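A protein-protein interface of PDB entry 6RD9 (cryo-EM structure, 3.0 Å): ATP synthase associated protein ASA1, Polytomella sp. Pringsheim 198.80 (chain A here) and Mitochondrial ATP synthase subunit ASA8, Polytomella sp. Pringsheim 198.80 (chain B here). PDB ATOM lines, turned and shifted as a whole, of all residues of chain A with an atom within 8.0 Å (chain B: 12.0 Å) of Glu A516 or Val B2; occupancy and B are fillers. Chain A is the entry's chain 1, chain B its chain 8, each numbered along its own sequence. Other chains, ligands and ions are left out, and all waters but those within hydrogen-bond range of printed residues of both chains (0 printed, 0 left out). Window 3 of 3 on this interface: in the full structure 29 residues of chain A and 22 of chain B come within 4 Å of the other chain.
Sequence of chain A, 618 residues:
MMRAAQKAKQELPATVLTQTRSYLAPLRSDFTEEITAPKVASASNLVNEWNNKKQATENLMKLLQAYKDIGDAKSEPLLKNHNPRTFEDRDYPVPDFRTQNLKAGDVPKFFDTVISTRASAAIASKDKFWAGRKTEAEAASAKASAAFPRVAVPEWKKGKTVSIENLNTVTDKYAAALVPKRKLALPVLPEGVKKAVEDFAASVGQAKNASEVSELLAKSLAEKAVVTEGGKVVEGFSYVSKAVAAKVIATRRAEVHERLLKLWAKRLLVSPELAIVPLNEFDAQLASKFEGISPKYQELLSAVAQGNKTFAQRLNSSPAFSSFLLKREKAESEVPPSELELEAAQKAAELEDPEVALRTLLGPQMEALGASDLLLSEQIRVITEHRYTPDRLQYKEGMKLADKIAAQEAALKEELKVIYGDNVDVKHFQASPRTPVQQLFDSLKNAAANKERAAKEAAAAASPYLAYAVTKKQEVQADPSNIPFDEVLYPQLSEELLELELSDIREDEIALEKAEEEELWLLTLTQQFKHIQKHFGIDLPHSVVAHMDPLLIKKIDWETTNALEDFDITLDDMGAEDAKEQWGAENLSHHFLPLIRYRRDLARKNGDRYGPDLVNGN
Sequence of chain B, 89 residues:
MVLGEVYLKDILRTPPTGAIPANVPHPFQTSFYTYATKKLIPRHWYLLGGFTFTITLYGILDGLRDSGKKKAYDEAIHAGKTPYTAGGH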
ATOM      1  N   ARG A 259     -27.290  27.843   5.289  1.00  0.00           N
ATOM      2  CA  ARG A 259     -27.260  26.915   6.405  1.00  0.00           C
ATOM      3  C   ARG A 259     -27.208  25.481   5.937  1.00  0.00           C
ATOM      4  O   ARG A 259     -26.735  24.619   6.669  1.00  0.00           O
ATOM      5  CB  ARG A 259     -28.463  27.104   7.296  1.00  0.00           C
ATOM      6  CG  ARG A 259     -28.414  28.366   8.035  1.00  0.00           C
ATOM      7  CD  ARG A 259     -29.447  28.378   9.097  1.00  0.00           C
ATOM      8  NE  ARG A 259     -29.252  27.311  10.052  1.00  0.00           N
ATOM      9  CZ  ARG A 259     -29.799  27.311  11.254  1.00  0.00           C
ATOM     10  NH1 ARG A 259     -29.576  26.314  12.082  1.00  0.00           N
ATOM     11  NH2 ARG A 259     -30.559  28.322  11.634  1.00  0.00           N
ATOM     12  N   LEU A 260     -27.709  25.197   4.749  1.00  0.00           N
ATOM     13  CA  LEU A 260     -27.514  23.877   4.182  1.00  0.00           C
ATOM     14  C   LEU A 260     -26.077  23.696   3.739  1.00  0.00           C
ATOM     15  O   LEU A 260     -25.515  22.607   3.862  1.00  0.00           O
ATOM     16  CB  LEU A 260     -28.461  23.673   3.010  1.00  0.00           C
ATOM     17  CG  LEU A 260     -28.332  22.363   2.257  1.00  0.00           C
ATOM     18  CD1 LEU A 260     -29.210  21.327   2.870  1.00  0.00           C
ATOM     19  CD2 LEU A 260     -28.648  22.549   0.824  1.00  0.00           C
ATOM     20  N   LYS A 262     -23.565  25.229   5.147  1.00  0.00           N
ATOM     21  CA  LYS A 262     -22.801  25.134   6.379  1.00  0.00           C
ATOM     22  C   LYS A 262     -23.059  23.838   7.111  1.00  0.00           C
ATOM     23  O   LYS A 262     -22.206  23.406   7.877  1.00  0.00           O
ATOM     24  CB  LYS A 262     -23.129  26.290   7.307  1.00  0.00           C
ATOM     25  CG  LYS A 262     -22.413  27.549   6.994  1.00  0.00           C
ATOM     26  CD  LYS A 262     -23.001  28.672   7.772  1.00  0.00           C
ATOM     27  CE  LYS A 262     -22.329  29.962   7.428  1.00  0.00           C
ATOM     28  NZ  LYS A 262     -22.808  31.028   8.333  1.00  0.00           N
ATOM     29  N   LEU A 263     -24.233  23.237   6.930  1.00  0.00           N
ATOM     30  CA  LEU A 263     -24.491  21.922   7.498  1.00  0.00           C
ATOM     31  C   LEU A 263     -23.563  20.901   6.894  1.00  0.00           C
ATOM     32  O   LEU A 263     -22.823  20.234   7.604  1.00  0.00           O
ATOM     33  CB  LEU A 263     -25.925  21.494   7.241  1.00  0.00           C
ATOM     34  CG  LEU A 263     -26.472  20.362   8.086  1.00  0.00           C
ATOM     35  CD1 LEU A 263     -27.073  20.937   9.326  1.00  0.00           C
ATOM     36  CD2 LEU A 263     -27.457  19.526   7.347  1.00  0.00           C
ATOM     37  N   LYS A 266     -19.646  21.038   7.752  1.00  0.00           N
ATOM     38  CA  LYS A 266     -19.144  20.368   8.939  1.00  0.00           C
ATOM     39  C   LYS A 266     -19.097  18.867   8.762  1.00  0.00           C
ATOM     40  O   LYS A 266     -18.218  18.208   9.307  1.00  0.00           O
ATOM     41  CB  LYS A 266     -20.011  20.704  10.133  1.00  0.00           C
ATOM     42  CG  LYS A 266     -20.319  22.133  10.266  1.00  0.00           C
ATOM     43  CD  LYS A 266     -21.471  22.299  11.166  1.00  0.00           C
ATOM     44  CE  LYS A 266     -21.941  23.704  11.178  1.00  0.00           C
ATOM     45  NZ  LYS A 266     -23.186  23.814  11.943  1.00  0.00           N
ATOM     46  N   ARG A 267     -20.025  18.309   8.021  1.00  0.00           N
ATOM     47  CA  ARG A 267     -20.102  16.871   7.902  1.00  0.00           C
ATOM     48  C   ARG A 267     -19.070  16.338   6.944  1.00  0.00           C
ATOM     49  O   ARG A 267     -18.766  15.153   6.986  1.00  0.00           O
ATOM     50  CB  ARG A 267     -21.487  16.450   7.433  1.00  0.00           C
ATOM     51  CG  ARG A 267     -22.473  16.165   8.512  1.00  0.00           C
ATOM     52  CD  ARG A 267     -22.933  17.411   9.128  1.00  0.00           C
ATOM     53  NE  ARG A 267     -24.069  17.235   9.984  1.00  0.00           N
ATOM     54  CZ  ARG A 267     -24.517  18.172  10.789  1.00  0.00           C
ATOM     55  NH1 ARG A 267     -23.907  19.329  10.837  1.00  0.00           N
ATOM     56  NH2 ARG A 267     -25.552  17.942  11.559  1.00  0.00           N
ATOM     57  N   GLU A 509     -35.753  25.398   7.346  1.00  0.00           N
ATOM     58  CA  GLU A 509     -34.852  25.915   8.355  1.00  0.00           C
ATOM     59  C   GLU A 509     -35.046  25.218   9.685  1.00  0.00           C
ATOM     60  O   GLU A 509     -34.119  25.172  10.489  1.00  0.00           O
ATOM     61  CB  GLU A 509     -35.059  27.408   8.521  1.00  0.00           C
ATOM     62  CG  GLU A 509     -33.869  28.131   9.049  1.00  0.00           C
ATOM     63  CD  GLU A 509     -34.224  29.513   9.516  1.00  0.00           C
ATOM     64  OE1 GLU A 509     -35.336  29.680  10.057  1.00  0.00           O
ATOM     65  OE2 GLU A 509     -33.394  30.429   9.350  1.00  0.00           O
ATOM     66  N   ILE A 510     -36.239  24.699   9.951  1.00  0.00           N
ATOM     67  CA  ILE A 510     -36.431  23.856  11.121  1.00  0.00           C
ATOM     68  C   ILE A 510     -35.748  22.512  10.920  1.00  0.00           C
ATOM     69  O   ILE A 510     -35.230  21.920  11.870  1.00  0.00           O
ATOM     70  CB  ILE A 510     -37.936  23.729  11.402  1.00  0.00           C
ATOM     71  CG1 ILE A 510     -38.496  25.068  11.842  1.00  0.00           C
ATOM     72  CG2 ILE A 510     -38.235  22.738  12.485  1.00  0.00           C
ATOM     73  CD1 ILE A 510     -39.984  25.083  11.930  1.00  0.00           C
ATOM     74  N   ALA A 511     -35.681  22.030   9.683  1.00  0.00           N
ATOM     75  CA  ALA A 511     -35.001  20.770   9.415  1.00  0.00           C
ATOM     76  C   ALA A 511     -33.496  20.882   9.574  1.00  0.00           C
ATOM     77  O   ALA A 511     -32.827  19.871   9.783  1.00  0.00           O
ATOM     78  CB  ALA A 511     -35.333  20.285   8.014  1.00  0.00           C
ATOM     79  N   LEU A 512     -32.940  22.080   9.454  1.00  0.00           N
ATOM     80  CA  LEU A 512     -31.510  22.247   9.652  1.00  0.00           C
ATOM     81  C   LEU A 512     -31.181  22.633  11.077  1.00  0.00           C
ATOM     82  O   LEU A 512     -30.032  22.517  11.489  1.00  0.00           O
ATOM     83  CB  LEU A 512     -30.956  23.299   8.707  1.00  0.00           C
ATOM     84  CG  LEU A 512     -31.134  23.018   7.230  1.00  0.00           C
ATOM     85  CD1 LEU A 512     -30.553  24.149   6.471  1.00  0.00           C
ATOM     86  CD2 LEU A 512     -30.477  21.742   6.840  1.00  0.00           C
ATOM     87  N   GLU A 513     -32.143  23.161  11.819  1.00  0.00           N
ATOM     88  CA  GLU A 513     -31.904  23.406  13.229  1.00  0.00           C
ATOM     89  C   GLU A 513     -32.002  22.124  14.022  1.00  0.00           C
ATOM     90  O   GLU A 513     -31.395  22.007  15.085  1.00  0.00           O
ATOM     91  CB  GLU A 513     -32.898  24.422  13.772  1.00  0.00           C
ATOM     92  CG  GLU A 513     -32.658  25.843  13.344  1.00  0.00           C
ATOM     93  CD  GLU A 513     -33.727  26.788  13.860  1.00  0.00           C
ATOM     94  OE1 GLU A 513     -33.575  28.018  13.696  1.00  0.00           O
ATOM     95  OE2 GLU A 513     -34.721  26.302  14.439  1.00  0.00           O
ATOM     96  N   LYS A 514     -32.793  21.173  13.544  1.00  0.00           N
ATOM     97  CA  LYS A 514     -32.862  19.876  14.189  1.00  0.00           C
ATOM     98  C   LYS A 514     -31.639  19.043  13.880  1.00  0.00           C
ATOM     99  O   LYS A 514     -31.226  18.228  14.701  1.00  0.00           O
ATOM    100  CB  LYS A 514     -34.107  19.134  13.734  1.00  0.00           C
ATOM    101  CG  LYS A 514     -35.377  19.606  14.350  1.00  0.00           C
ATOM    102  CD  LYS A 514     -36.531  18.887  13.730  1.00  0.00           C
ATOM    103  CE  LYS A 514     -37.830  19.384  14.291  1.00  0.00           C
ATOM    104  NZ  LYS A 514     -38.981  18.835  13.537  1.00  0.00           N
ATOM    105  N   ALA A 515     -31.052  19.227  12.710  1.00  0.00           N
ATOM    106  CA  ALA A 515     -29.901  18.442  12.310  1.00  0.00           C
ATOM    107  C   ALA A 515     -28.642  18.832  13.043  1.00  0.00           C
ATOM    108  O   ALA A 515     -27.673  18.081  13.001  1.00  0.00           O
ATOM    109  CB  ALA A 515     -29.652  18.580  10.819  1.00  0.00           C
ATOM    110  N   GLU A 516     -28.620  19.980  13.698  1.00  0.00           N
ATOM    111  CA  GLU A 516     -27.428  20.449  14.375  1.00  0.00           C
ATOM    112  C   GLU A 516     -27.615  20.517  15.877  1.00  0.00           C
ATOM    113  O   GLU A 516     -26.835  21.167  16.571  1.00  0.00           O
ATOM    114  CB  GLU A 516     -27.003  21.798  13.810  1.00  0.00           C
ATOM    115  CG  GLU A 516     -27.924  22.943  14.086  1.00  0.00           C
ATOM    116  CD  GLU A 516     -27.569  24.152  13.262  1.00  0.00           C
ATOM    117  OE1 GLU A 516     -27.121  23.971  12.114  1.00  0.00           O
ATOM    118  OE2 GLU A 516     -27.741  25.283  13.751  1.00  0.00           O
ATOM    119  N   GLU A 517     -28.607  19.823  16.398  1.00  0.00           N
ATOM    120  CA  GLU A 517     -28.841  19.835  17.829  1.00  0.00           C
ATOM    121  C   GLU A 517     -27.870  18.924  18.561  1.00  0.00           C
ATOM    122  O   GLU A 517     -27.295  19.308  19.580  1.00  0.00           O
ATOM    123  CB  GLU A 517     -30.279  19.430  18.098  1.00  0.00           C
ATOM    124  CG  GLU A 517     -30.589  19.249  19.527  1.00  0.00           C
ATOM    125  CD  GLU A 517     -31.952  18.674  19.741  1.00  0.00           C
ATOM    126  OE1 GLU A 517     -32.597  18.300  18.743  1.00  0.00           O
ATOM    127  OE2 GLU A 517     -32.381  18.591  20.905  1.00  0.00           O
ATOM    128  N   GLU A 518     -27.676  17.714  18.062  1.00  0.00           N
ATOM    129  CA  GLU A 518     -26.758  16.754  18.652  1.00  0.00           C
ATOM    130  C   GLU A 518     -25.656  16.396  17.682  1.00  0.00           C
ATOM    131  O   GLU A 518     -25.213  15.262  17.620  1.00  0.00           O
ATOM    132  CB  GLU A 518     -27.486  15.493  19.077  1.00  0.00           C
ATOM    133  CG  GLU A 518     -28.748  15.744  19.820  1.00  0.00           C
ATOM    134  CD  GLU A 518     -29.680  14.582  19.725  1.00  0.00           C
ATOM    135  OE1 GLU A 518     -29.304  13.590  19.075  1.00  0.00           O
ATOM    136  OE2 GLU A 518     -30.784  14.652  20.294  1.00  0.00           O
ATOM    137  N   GLU A 519     -25.234  17.351  16.877  1.00  0.00           N
ATOM    138  CA  GLU A 519     -24.186  17.090  15.918  1.00  0.00           C
ATOM    139  C   GLU A 519     -22.811  17.175  16.522  1.00  0.00           C
ATOM    140  O   GLU A 519     -21.853  16.772  15.872  1.00  0.00           O
ATOM    141  CB  GLU A 519     -24.261  18.072  14.772  1.00  0.00           C
ATOM    142  CG  GLU A 519     -23.989  19.463  15.235  1.00  0.00           C
ATOM    143  CD  GLU A 519     -23.650  20.383  14.127  1.00  0.00           C
ATOM    144  OE1 GLU A 519     -23.247  19.883  13.070  1.00  0.00           O
ATOM    145  OE2 GLU A 519     -23.775  21.606  14.315  1.00  0.00           O
ATOM    146  N   LEU A 520     -22.664  17.728  17.720  1.00  0.00           N
ATOM    147  CA  LEU A 520     -21.340  17.733  18.316  1.00  0.00           C
ATOM    148  C   LEU A 520     -20.982  16.350  18.797  1.00  0.00           C
ATOM    149  O   LEU A 520     -19.848  15.905  18.632  1.00  0.00           O
ATOM    150  CB  LEU A 520     -21.263  18.717  19.467  1.00  0.00           C
ATOM    151  CG  LEU A 520     -19.853  18.858  20.004  1.00  0.00           C
ATOM    152  CD1 LEU A 520     -18.974  19.333  18.917  1.00  0.00           C
ATOM    153  CD2 LEU A 520     -19.809  19.788  21.121  1.00  0.00           C
ATOM    154  N   TRP A 521     -21.948  15.642  19.344  1.00  0.00           N
ATOM    155  CA  TRP A 521     -21.685  14.317  19.858  1.00  0.00           C
ATOM    156  C   TRP A 521     -21.505  13.315  18.741  1.00  0.00           C
ATOM    157  O   TRP A 521     -20.628  12.465  18.817  1.00  0.00           O
ATOM    158  CB  TRP A 521     -22.816  13.903  20.769  1.00  0.00           C
ATOM    159  CG  TRP A 521     -22.808  12.511  21.142  1.00  0.00           C
ATOM    160  CD1 TRP A 521     -21.973  11.911  21.993  1.00  0.00           C
ATOM    161  CD2 TRP A 521     -23.723  11.527  20.712  1.00  0.00           C
ATOM    162  NE1 TRP A 521     -22.288  10.602  22.119  1.00  0.00           N
ATOM    163  CE2 TRP A 521     -23.364  10.340  21.326  1.00  0.00           C
ATOM    164  CE3 TRP A 521     -24.808  11.536  19.850  1.00  0.00           C
ATOM    165  CZ2 TRP A 521     -24.045   9.177  21.117  1.00  0.00           C
ATOM    166  CZ3 TRP A 521     -25.474  10.389  19.639  1.00  0.00           C
ATOM    167  CH2 TRP A 521     -25.101   9.222  20.275  1.00  0.00           C
ATOM    168  N   LEU A 523     -20.446  13.793  15.733  1.00  0.00           N
ATOM    169  CA  LEU A 523     -19.263  14.039  14.935  1.00  0.00           C
ATOM    170  C   LEU A 523     -17.993  13.949  15.747  1.00  0.00           C
ATOM    171  O   LEU A 523     -16.916  13.882  15.167  1.00  0.00           O
ATOM    172  CB  LEU A 523     -19.340  15.410  14.271  1.00  0.00           C
ATOM    173  CG  LEU A 523     -20.322  15.755  13.154  1.00  0.00           C
ATOM    174  CD1 LEU A 523     -20.331  17.234  12.943  1.00  0.00           C
ATOM    175  CD2 LEU A 523     -19.976  15.065  11.884  1.00  0.00           C
ATOM    176  N   TYR A 598     -27.671  14.900  27.879  1.00  0.00           N
ATOM    177  CA  TYR A 598     -28.279  16.030  27.201  1.00  0.00           C
ATOM    178  C   TYR A 598     -29.771  15.853  27.069  1.00  0.00           C
ATOM    179  O   TYR A 598     -30.528  16.791  27.305  1.00  0.00           O
ATOM    180  CB  TYR A 598     -27.681  16.202  25.823  1.00  0.00           C
ATOM    181  CG  TYR A 598     -28.423  17.184  24.979  1.00  0.00           C
ATOM    182  CD1 TYR A 598     -28.494  18.504  25.344  1.00  0.00           C
ATOM    183  CD2 TYR A 598     -29.035  16.794  23.807  1.00  0.00           C
ATOM    184  CE1 TYR A 598     -29.152  19.400  24.584  1.00  0.00           C
ATOM    185  CE2 TYR A 598     -29.702  17.692  23.041  1.00  0.00           C
ATOM    186  CZ  TYR A 598     -29.747  18.990  23.434  1.00  0.00           C
ATOM    187  OH  TYR A 598     -30.413  19.912  22.686  1.00  0.00           O
ATOM    188  N   LEU A 602     -32.786  18.043  28.652  1.00  0.00           N
ATOM    189  CA  LEU A 602     -33.922  18.568  27.914  1.00  0.00           C
ATOM    190  C   LEU A 602     -35.203  18.276  28.663  1.00  0.00           C
ATOM    191  O   LEU A 602     -35.950  19.190  29.013  1.00  0.00           O
ATOM    192  CB  LEU A 602     -33.993  17.948  26.528  1.00  0.00           C
ATOM    193  CG  LEU A 602     -33.231  18.609  25.407  1.00  0.00           C
ATOM    194  CD1 LEU A 602     -33.681  18.025  24.101  1.00  0.00           C
ATOM    195  CD2 LEU A 602     -33.467  20.074  25.435  1.00  0.00           C
ATOM    196  N   VAL B   2     -28.462  23.128  22.072  1.00  0.00           N
ATOM    197  CA  VAL B   2     -27.695  22.142  21.341  1.00  0.00           C
ATOM    198  C   VAL B   2     -26.876  21.331  22.314  1.00  0.00           C
ATOM    199  O   VAL B   2     -26.774  21.679  23.482  1.00  0.00           O
ATOM    200  CB  VAL B   2     -26.801  22.801  20.305  1.00  0.00           C
ATOM    201  CG1 VAL B   2     -27.615  23.652  19.390  1.00  0.00           C
ATOM    202  CG2 VAL B   2     -25.760  23.639  20.986  1.00  0.00           C
ATOM    203  N   LEU B   3     -26.293  20.242  21.834  1.00  0.00           N
ATOM    204  CA  LEU B   3     -25.322  19.504  22.622  1.00  0.00           C
ATOM    205  C   LEU B   3     -24.004  20.243  22.506  1.00  0.00           C
ATOM    206  O   LEU B   3     -23.440  20.343  21.416  1.00  0.00           O
ATOM    207  CB  LEU B   3     -25.203  18.076  22.122  1.00  0.00           C
ATOM    208  CG  LEU B   3     -24.782  17.004  23.100  1.00  0.00           C
ATOM    209  CD1 LEU B   3     -25.415  15.749  22.663  1.00  0.00           C
ATOM    210  CD2 LEU B   3     -23.302  16.850  23.118  1.00  0.00           C
ATOM    211  N   GLY B   4     -23.537  20.790  23.611  1.00  0.00           N
ATOM    212  CA  GLY B   4     -22.585  21.866  23.525  1.00  0.00           C
ATOM    213  C   GLY B   4     -21.296  21.787  24.300  1.00  0.00           C
ATOM    214  O   GLY B   4     -20.980  22.746  25.008  1.00  0.00           O
ATOM    215  N   GLU B   5     -20.624  20.638  24.287  1.00  0.00           N
ATOM    216  CA  GLU B   5     -19.239  20.452  24.731  1.00  0.00           C
ATOM    217  C   GLU B   5     -19.060  20.513  26.237  1.00  0.00           C
ATOM    218  O   GLU B   5     -17.999  20.163  26.748  1.00  0.00           O
ATOM    219  CB  GLU B   5     -18.293  21.458  24.077  1.00  0.00           C
ATOM    220  CG  GLU B   5     -16.913  20.938  23.850  1.00  0.00           C
ATOM    221  CD  GLU B   5     -15.899  22.045  23.802  1.00  0.00           C
ATOM    222  OE1 GLU B   5     -16.275  23.172  23.431  1.00  0.00           O
ATOM    223  OE2 GLU B   5     -14.728  21.800  24.153  1.00  0.00           O
ATOM    224  N   VAL B   6     -20.079  20.909  26.978  1.00  0.00           N
ATOM    225  CA  VAL B   6     -20.037  20.677  28.405  1.00  0.00           C
ATOM    226  C   VAL B   6     -20.530  19.271  28.691  1.00  0.00           C
ATOM    227  O   VAL B   6     -20.264  18.732  29.771  1.00  0.00           O
ATOM    228  CB  VAL B   6     -20.844  21.758  29.143  1.00  0.00           C
ATOM    229  CG1 VAL B   6     -22.317  21.512  29.030  1.00  0.00           C
ATOM    230  CG2 VAL B   6     -20.411  21.882  30.581  1.00  0.00           C
ATOM    231  N   TYR B   7     -21.199  18.641  27.736  1.00  0.00           N
ATOM    232  CA  TYR B   7     -21.642  17.275  27.894  1.00  0.00           C
ATOM    233  C   TYR B   7     -20.591  16.284  27.464  1.00  0.00           C
ATOM    234  O   TYR B   7     -20.601  15.152  27.943  1.00  0.00           O
ATOM    235  CB  TYR B   7     -22.919  17.039  27.100  1.00  0.00           C
ATOM    236  CG  TYR B   7     -24.071  17.847  27.593  1.00  0.00           C
ATOM    237  CD1 TYR B   7     -24.724  17.500  28.754  1.00  0.00           C
ATOM    238  CD2 TYR B   7     -24.511  18.949  26.901  1.00  0.00           C
ATOM    239  CE1 TYR B   7     -25.775  18.227  29.212  1.00  0.00           C
ATOM    240  CE2 TYR B   7     -25.558  19.688  27.352  1.00  0.00           C
ATOM    241  CZ  TYR B   7     -26.187  19.323  28.507  1.00  0.00           C
ATOM    242  OH  TYR B   7     -27.243  20.064  28.961  1.00  0.00           O
ATOM    243  N   LEU B   8     -19.691  16.679  26.587  1.00  0.00           N
ATOM    244  CA  LEU B   8     -18.594  15.834  26.164  1.00  0.00           C
ATOM    245  C   LEU B   8     -17.351  16.016  27.004  1.00  0.00           C
ATOM    246  O   LEU B   8     -16.313  15.467  26.652  1.00  0.00           O
ATOM    247  CB  LEU B   8     -18.219  16.132  24.725  1.00  0.00           C
ATOM    248  CG  LEU B   8     -19.146  15.999  23.547  1.00  0.00           C
ATOM    249  CD1 LEU B   8     -18.383  16.588  22.478  1.00  0.00           C
ATOM    250  CD2 LEU B   8     -19.345  14.600  23.215  1.00  0.00           C
ATOM    251  N   LYS B   9     -17.402  16.799  28.069  1.00  0.00           N
ATOM    252  CA  LYS B   9     -16.195  17.100  28.819  1.00  0.00           C
ATOM    253  C   LYS B   9     -15.780  15.909  29.657  1.00  0.00           C
ATOM    254  O   LYS B   9     -16.585  15.370  30.417  1.00  0.00           O
ATOM    255  CB  LYS B   9     -16.408  18.304  29.718  1.00  0.00           C
ATOM    256  CG  LYS B   9     -15.137  18.835  30.304  1.00  0.00           C
ATOM    257  CD  LYS B   9     -15.410  19.852  31.363  1.00  0.00           C
ATOM    258  CE  LYS B   9     -15.817  19.198  32.660  1.00  0.00           C
ATOM    259  NZ  LYS B   9     -14.650  18.732  33.439  1.00  0.00           N
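O of Glu A517 sits at hydrogen-bond distance from N of Leu B3, 2.6 Å away.
The guanidinium group (NH1) of Arg A259 is in salt-bridge range of the side-chain carboxylate (OE2) of Glu A516.
OE2 of Glu A517 lies within hydrogen-bond range of OH of Tyr A598, at 3.0 Å.
OE1 of Glu A516 lies within salt-bridge range of NZ of Lys A266.
Among the printed residues, pairs that only touch across the chains: Leu A520 with Leu B3 (3.3 Å), Glu A517 with Val B2 (3.4 Å), Leu A520 with Glu B5 (3.4 Å), Tyr A598 with Val B2 (3.5 Å), Leu A520 with Leu B8 (3.7 Å), Trp A521 with Leu B3 (3.7 Å), Tyr A598 with Tyr B7 (3.7 Å), Glu A516 with Val B2 (3.8 Å), Tyr A598 with Leu B3 (3.9 Å) and Trp A521 with Leu B8 (3.95 Å).
No residue of chain B comes within 4 Å of Arg A259.
No residue of chain B comes within 4 Å of Leu A263.
No residue of chain B comes within 4 Å of Leu A512.
Glu A513 touches none of the printed residues of chain B.
Glu A516 touches just one residue of chain B: Val B2.
Printed residues of chain B within 4 Å of Leu A520: Leu B3, Glu B5 and Leu B8.
Printed residues of chain B within 4 Å of Trp A521: Leu B3 and Leu B8.
Of chain A, only Glu A516 (3.8 Å), Glu A517 (3.4 Å) and Tyr A598 (3.5 Å) come within 4 Å of Val B2.
Printed residues of chain A within 4 Å of Leu B8: Leu A520 (3.7 Å) and Trp A521 (3.95 Å).
The nearest residue of chain B that does not touch Glu A516 is Leu B3 (5.4 Å).
The nearest residue of chain A that does not touch Val B2 is Glu A518 (5.5 Å).
Of the 8 printed residues of chain B, 5 touch a printed residue of chain A.
Hydrophobic or aromatic side chains of chain B within 4 Å of the printed part of chain A: Val B2, Leu B3, Tyr B7 and Leu B8.
Printed residues of chain A that touch a printed residue of chain B: Glu A516, Glu A517, Leu A520, Trp A521 and Tyr A598.
Among the printed residues, no Asp or Glu carboxylate lies within 4 Å of a Lys or Arg side-chain nitrogen of the other chain.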
